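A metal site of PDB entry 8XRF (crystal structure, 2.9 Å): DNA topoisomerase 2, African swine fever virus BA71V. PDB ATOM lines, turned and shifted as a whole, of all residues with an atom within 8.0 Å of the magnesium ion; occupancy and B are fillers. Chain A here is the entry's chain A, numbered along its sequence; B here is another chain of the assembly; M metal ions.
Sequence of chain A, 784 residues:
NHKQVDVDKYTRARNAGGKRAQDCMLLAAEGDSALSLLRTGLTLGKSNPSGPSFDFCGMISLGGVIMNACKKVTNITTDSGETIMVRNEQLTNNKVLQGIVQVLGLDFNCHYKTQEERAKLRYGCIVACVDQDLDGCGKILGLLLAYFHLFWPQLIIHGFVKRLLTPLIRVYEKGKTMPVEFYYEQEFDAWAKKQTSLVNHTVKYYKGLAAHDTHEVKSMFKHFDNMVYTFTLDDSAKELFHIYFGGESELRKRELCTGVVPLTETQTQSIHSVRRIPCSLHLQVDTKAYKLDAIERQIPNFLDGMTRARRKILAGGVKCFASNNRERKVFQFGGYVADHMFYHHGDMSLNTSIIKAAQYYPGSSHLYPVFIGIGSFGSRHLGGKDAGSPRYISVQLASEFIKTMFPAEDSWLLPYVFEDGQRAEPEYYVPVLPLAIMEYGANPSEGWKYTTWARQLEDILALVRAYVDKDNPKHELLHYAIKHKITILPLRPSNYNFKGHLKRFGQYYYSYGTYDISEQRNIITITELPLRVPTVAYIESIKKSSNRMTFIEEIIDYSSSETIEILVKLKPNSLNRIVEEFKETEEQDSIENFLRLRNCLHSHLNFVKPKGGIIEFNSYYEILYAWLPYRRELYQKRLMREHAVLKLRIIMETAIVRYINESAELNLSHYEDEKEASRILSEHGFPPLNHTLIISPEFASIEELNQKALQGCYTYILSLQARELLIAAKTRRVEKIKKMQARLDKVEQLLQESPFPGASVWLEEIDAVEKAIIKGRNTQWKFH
The magnesium ion is bound by the side-chain amide oxygen (OD1) of Asn 667 of chain B (2.0 Å), the side-chain amide oxygen (OD1) of Asn 667 of chain A (2.1 Å) and the backbone carbonyl oxygen (O) of Ala 664 of chain A (2.5 Å). The magnesium ion has three donor atoms within binding distance. Slightly farther from the magnesium ion lies the backbone carbonyl oxygen (O) of Ala 664 of chain B (2.6 Å).
Of the 18 residues printed, 4 come within 4 Å of the magnesium ion. The nearest printed residue that does not touch the magnesium ion is Glu 665 of chain A (4.6 Å).
The side-chain amide nitrogen (ND2) of Asn 667 of chain B lies within hydrogen-bond range of the backbone carbonyl oxygen (O) of Ala 664 of chain B (3.3 Å). The backbone carbonyl oxygen (O) of Asn 667 of chain A lies within hydrogen-bond range of a ring nitrogen (ND1) of His 670 of chain A (3.2 Å). ND2 of Asn 667 of chain A lies within hydrogen-bond range of O of Glu 665 of chain A (3.4 Å).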
ATOM      1  N   GLU A 662      -2.253  18.584   2.044  1.00  0.00           N
ATOM      2  CA  GLU A 662      -3.208  17.890   1.189  1.00  0.00           C
ATOM      3  C   GLU A 662      -2.600  17.483  -0.155  1.00  0.00           C
ATOM      4  O   GLU A 662      -3.313  16.947  -1.006  1.00  0.00           O
ATOM      5  CB  GLU A 662      -4.436  18.758   0.947  1.00  0.00           C
ATOM      6  CG  GLU A 662      -5.436  18.796   2.093  1.00  0.00           C
ATOM      7  CD  GLU A 662      -6.869  18.673   1.620  1.00  0.00           C
ATOM      8  OE1 GLU A 662      -7.260  17.558   1.217  1.00  0.00           O
ATOM      9  OE2 GLU A 662      -7.595  19.679   1.649  1.00  0.00           O
ATOM     10  N   SER A 663      -1.296  17.696  -0.353  1.00  0.00           N
ATOM     11  CA  SER A 663      -0.721  17.440  -1.670  1.00  0.00           C
ATOM     12  C   SER A 663      -0.635  15.943  -1.969  1.00  0.00           C
ATOM     13  O   SER A 663      -0.737  15.548  -3.138  1.00  0.00           O
ATOM     14  CB  SER A 663       0.674  18.070  -1.760  1.00  0.00           C
ATOM     15  OG  SER A 663       1.535  17.563  -0.767  1.00  0.00           O
ATOM     16  N   ALA A 664      -0.453  15.109  -0.950  1.00  0.00           N
ATOM     17  CA  ALA A 664      -0.283  13.675  -1.187  1.00  0.00           C
ATOM     18  C   ALA A 664      -1.588  13.034  -1.652  1.00  0.00           C
ATOM     19  O   ALA A 664      -1.597  12.280  -2.623  1.00  0.00           O
ATOM     20  CB  ALA A 664       0.227  12.997   0.077  1.00  0.00           C
ATOM     21  N   GLU A 665      -2.700  13.321  -0.961  1.00  0.00           N
ATOM     22  CA  GLU A 665      -3.975  12.753  -1.378  1.00  0.00           C
ATOM     23  C   GLU A 665      -4.503  13.442  -2.623  1.00  0.00           C
ATOM     24  O   GLU A 665      -5.022  12.790  -3.530  1.00  0.00           O
ATOM     25  CB  GLU A 665      -4.988  12.882  -0.235  1.00  0.00           C
ATOM     26  CG  GLU A 665      -4.434  12.536   1.145  1.00  0.00           C
ATOM     27  CD  GLU A 665      -4.291  13.756   2.035  1.00  0.00           C
ATOM     28  OE1 GLU A 665      -3.600  14.713   1.620  1.00  0.00           O
ATOM     29  OE2 GLU A 665      -4.860  13.757   3.152  1.00  0.00           O
ATOM     30  N   LEU A 666      -4.372  14.771  -2.675  1.00  0.00           N
ATOM     31  CA  LEU A 666      -4.883  15.583  -3.788  1.00  0.00           C
ATOM     32  C   LEU A 666      -3.803  15.680  -4.866  1.00  0.00           C
ATOM     33  O   LEU A 666      -3.170  16.715  -5.086  1.00  0.00           O
ATOM     34  CB  LEU A 666      -5.314  16.953  -3.270  1.00  0.00           C
ATOM     35  CG  LEU A 666      -6.187  17.962  -3.993  1.00  0.00           C
ATOM     36  CD1 LEU A 666      -6.953  18.755  -2.945  1.00  0.00           C
ATOM     37  CD2 LEU A 666      -5.349  18.912  -4.837  1.00  0.00           C
ATOM     38  N   ASN A 667      -3.589  14.550  -5.551  1.00  0.00           N
ATOM     39  CA  ASN A 667      -2.499  14.414  -6.512  1.00  0.00           C
ATOM     40  C   ASN A 667      -2.764  15.264  -7.745  1.00  0.00           C
ATOM     41  O   ASN A 667      -3.618  14.933  -8.567  1.00  0.00           O
ATOM     42  CB  ASN A 667      -2.313  12.943  -6.892  1.00  0.00           C
ATOM     43  CG  ASN A 667      -1.820  12.092  -5.741  1.00  0.00           C
ATOM     44  OD1 ASN A 667      -0.716  12.291  -5.231  1.00  0.00           O
ATOM     45  ND2 ASN A 667      -2.645  11.134  -5.324  1.00  0.00           N
ATOM     46  N   LEU A 668      -2.033  16.370  -7.865  1.00  0.00           N
ATOM     47  CA  LEU A 668      -2.156  17.252  -9.026  1.00  0.00           C
ATOM     48  C   LEU A 668      -1.752  16.577 -10.336  1.00  0.00           C
ATOM     49  O   LEU A 668      -2.109  17.067 -11.407  1.00  0.00           O
ATOM     50  CB  LEU A 668      -1.311  18.502  -8.829  1.00  0.00           C
ATOM     51  CG  LEU A 668      -2.052  19.833  -8.746  1.00  0.00           C
ATOM     52  CD1 LEU A 668      -1.082  21.004  -8.628  1.00  0.00           C
ATOM     53  CD2 LEU A 668      -2.993  20.008  -9.920  1.00  0.00           C
ATOM     54  N   SER A 669      -0.990  15.472 -10.260  1.00  0.00           N
ATOM     55  CA  SER A 669      -0.543  14.779 -11.466  1.00  0.00           C
ATOM     56  C   SER A 669      -1.678  14.426 -12.420  1.00  0.00           C
ATOM     57  O   SER A 669      -1.488  14.404 -13.634  1.00  0.00           O
ATOM     58  CB  SER A 669       0.213  13.500 -11.080  1.00  0.00           C
ATOM     59  OG  SER A 669       1.177  13.760 -10.072  1.00  0.00           O
ATOM     60  N   HIS A 670      -2.881  14.146 -11.885  1.00  0.00           N
ATOM     61  CA  HIS A 670      -3.978  13.632 -12.697  1.00  0.00           C
ATOM     62  C   HIS A 670      -4.772  14.699 -13.424  1.00  0.00           C
ATOM     63  O   HIS A 670      -5.548  14.366 -14.319  1.00  0.00           O
ATOM     64  CB  HIS A 670      -4.949  12.806 -11.851  1.00  0.00           C
ATOM     65  CG  HIS A 670      -4.302  11.727 -11.052  1.00  0.00           C
ATOM     66  ND1 HIS A 670      -3.589  11.982  -9.906  1.00  0.00           N
ATOM     67  CD2 HIS A 670      -4.244  10.394 -11.244  1.00  0.00           C
ATOM     68  CE1 HIS A 670      -3.125  10.844  -9.413  1.00  0.00           C
ATOM     69  NE2 HIS A 670      -3.508   9.867 -10.208  1.00  0.00           N
ATOM     70  N   GLU B 662       5.522   9.235 -12.247  1.00  0.00           N
ATOM     71  CA  GLU B 662       5.750   8.558 -10.982  1.00  0.00           C
ATOM     72  C   GLU B 662       5.568   9.489  -9.778  1.00  0.00           C
ATOM     73  O   GLU B 662       5.884   9.106  -8.650  1.00  0.00           O
ATOM     74  CB  GLU B 662       7.150   7.936 -10.949  1.00  0.00           C
ATOM     75  CG  GLU B 662       7.245   6.604 -11.688  1.00  0.00           C
ATOM     76  CD  GLU B 662       8.666   6.115 -11.874  1.00  0.00           C
ATOM     77  OE1 GLU B 662       9.476   6.284 -10.933  1.00  0.00           O
ATOM     78  OE2 GLU B 662       8.971   5.562 -12.948  1.00  0.00           O
ATOM     79  N   SER B 663       5.064  10.705 -10.006  1.00  0.00           N
ATOM     80  CA  SER B 663       4.963  11.687  -8.937  1.00  0.00           C
ATOM     81  C   SER B 663       3.888  11.320  -7.923  1.00  0.00           C
ATOM     82  O   SER B 663       4.002  11.673  -6.740  1.00  0.00           O
ATOM     83  CB  SER B 663       4.677  13.074  -9.519  1.00  0.00           C
ATOM     84  OG  SER B 663       3.419  13.100 -10.170  1.00  0.00           O
ATOM     85  N   ALA B 664       2.836  10.620  -8.348  1.00  0.00           N
ATOM     86  CA  ALA B 664       1.722  10.325  -7.447  1.00  0.00           C
ATOM     87  C   ALA B 664       2.143   9.345  -6.360  1.00  0.00           C
ATOM     88  O   ALA B 664       1.831   9.551  -5.180  1.00  0.00           O
ATOM     89  CB  ALA B 664       0.545   9.762  -8.241  1.00  0.00           C
ATOM     90  N   GLU B 665       2.839   8.273  -6.725  1.00  0.00           N
ATOM     91  CA  GLU B 665       3.301   7.313  -5.727  1.00  0.00           C
ATOM     92  C   GLU B 665       4.445   7.875  -4.891  1.00  0.00           C
ATOM     93  O   GLU B 665       4.513   7.629  -3.686  1.00  0.00           O
ATOM     94  CB  GLU B 665       3.715   5.995  -6.399  1.00  0.00           C
ATOM     95  CG  GLU B 665       4.320   6.152  -7.777  1.00  0.00           C
ATOM     96  CD  GLU B 665       4.855   4.835  -8.315  1.00  0.00           C
ATOM     97  OE1 GLU B 665       4.863   3.850  -7.557  1.00  0.00           O
ATOM     98  OE2 GLU B 665       5.265   4.803  -9.497  1.00  0.00           O
ATOM     99  N   LEU B 666       5.348   8.631  -5.516  1.00  0.00           N
ATOM    100  CA  LEU B 666       6.517   9.165  -4.829  1.00  0.00           C
ATOM    101  C   LEU B 666       6.128  10.464  -4.123  1.00  0.00           C
ATOM    102  O   LEU B 666       6.508  11.573  -4.518  1.00  0.00           O
ATOM    103  CB  LEU B 666       7.660   9.408  -5.820  1.00  0.00           C
ATOM    104  CG  LEU B 666       8.619   8.284  -6.172  1.00  0.00           C
ATOM    105  CD1 LEU B 666       7.942   7.249  -7.049  1.00  0.00           C
ATOM    106  CD2 LEU B 666       9.853   8.854  -6.862  1.00  0.00           C
ATOM    107  N   ASN B 667       5.358  10.313  -3.050  1.00  0.00           N
ATOM    108  CA  ASN B 667       4.826  11.466  -2.348  1.00  0.00           C
ATOM    109  C   ASN B 667       5.962  12.174  -1.639  1.00  0.00           C
ATOM    110  O   ASN B 667       6.389  11.763  -0.560  1.00  0.00           O
ATOM    111  CB  ASN B 667       3.745  11.031  -1.354  1.00  0.00           C
ATOM    112  CG  ASN B 667       2.447  10.638  -2.023  1.00  0.00           C
ATOM    113  OD1 ASN B 667       1.807  11.445  -2.694  1.00  0.00           O
ATOM    114  ND2 ASN B 667       2.047   9.379  -1.853  1.00  0.00           N
ATOM    115  N   LEU B 668       6.464  13.255  -2.241  1.00  0.00           N
ATOM    116  CA  LEU B 668       7.489  14.056  -1.585  1.00  0.00           C
ATOM    117  C   LEU B 668       6.963  14.714  -0.326  1.00  0.00           C
ATOM    118  O   LEU B 668       7.749  15.105   0.543  1.00  0.00           O
ATOM    119  CB  LEU B 668       8.041  15.105  -2.545  1.00  0.00           C
ATOM    120  CG  LEU B 668       8.799  14.572  -3.756  1.00  0.00           C
ATOM    121  CD1 LEU B 668       9.414  15.704  -4.559  1.00  0.00           C
ATOM    122  CD2 LEU B 668       9.860  13.574  -3.328  1.00  0.00           C
ATOM    123  N   SER B 669       5.635  14.861  -0.218  1.00  0.00           N
ATOM    124  CA  SER B 669       5.021  15.429   0.971  1.00  0.00           C
ATOM    125  C   SER B 669       5.440  14.694   2.236  1.00  0.00           C
ATOM    126  O   SER B 669       5.526  15.317   3.306  1.00  0.00           O
ATOM    127  CB  SER B 669       3.488  15.400   0.834  1.00  0.00           C
ATOM    128  OG  SER B 669       3.107  15.500  -0.522  1.00  0.00           O
ATOM    129  N   HIS B 670       5.680  13.385   2.158  1.00  0.00           N
ATOM    130  CA  HIS B 670       5.943  12.597   3.353  1.00  0.00           C
ATOM    131  C   HIS B 670       7.413  12.598   3.774  1.00  0.00           C
ATOM    132  O   HIS B 670       7.706  12.347   4.938  1.00  0.00           O
ATOM    133  CB  HIS B 670       5.508  11.143   3.122  1.00  0.00           C
ATOM    134  CG  HIS B 670       4.044  10.994   2.837  1.00  0.00           C
ATOM    135  ND1 HIS B 670       3.118  11.981   3.112  1.00  0.00           N
ATOM    136  CD2 HIS B 670       3.345   9.973   2.289  1.00  0.00           C
ATOM    137  CE1 HIS B 670       1.916  11.580   2.758  1.00  0.00           C
ATOM    138  NE2 HIS B 670       2.015  10.360   2.252  1.00  0.00           N
HETATM  139 MG    MG M   1       0.151  11.027  -3.799  1.00  0.00          MG
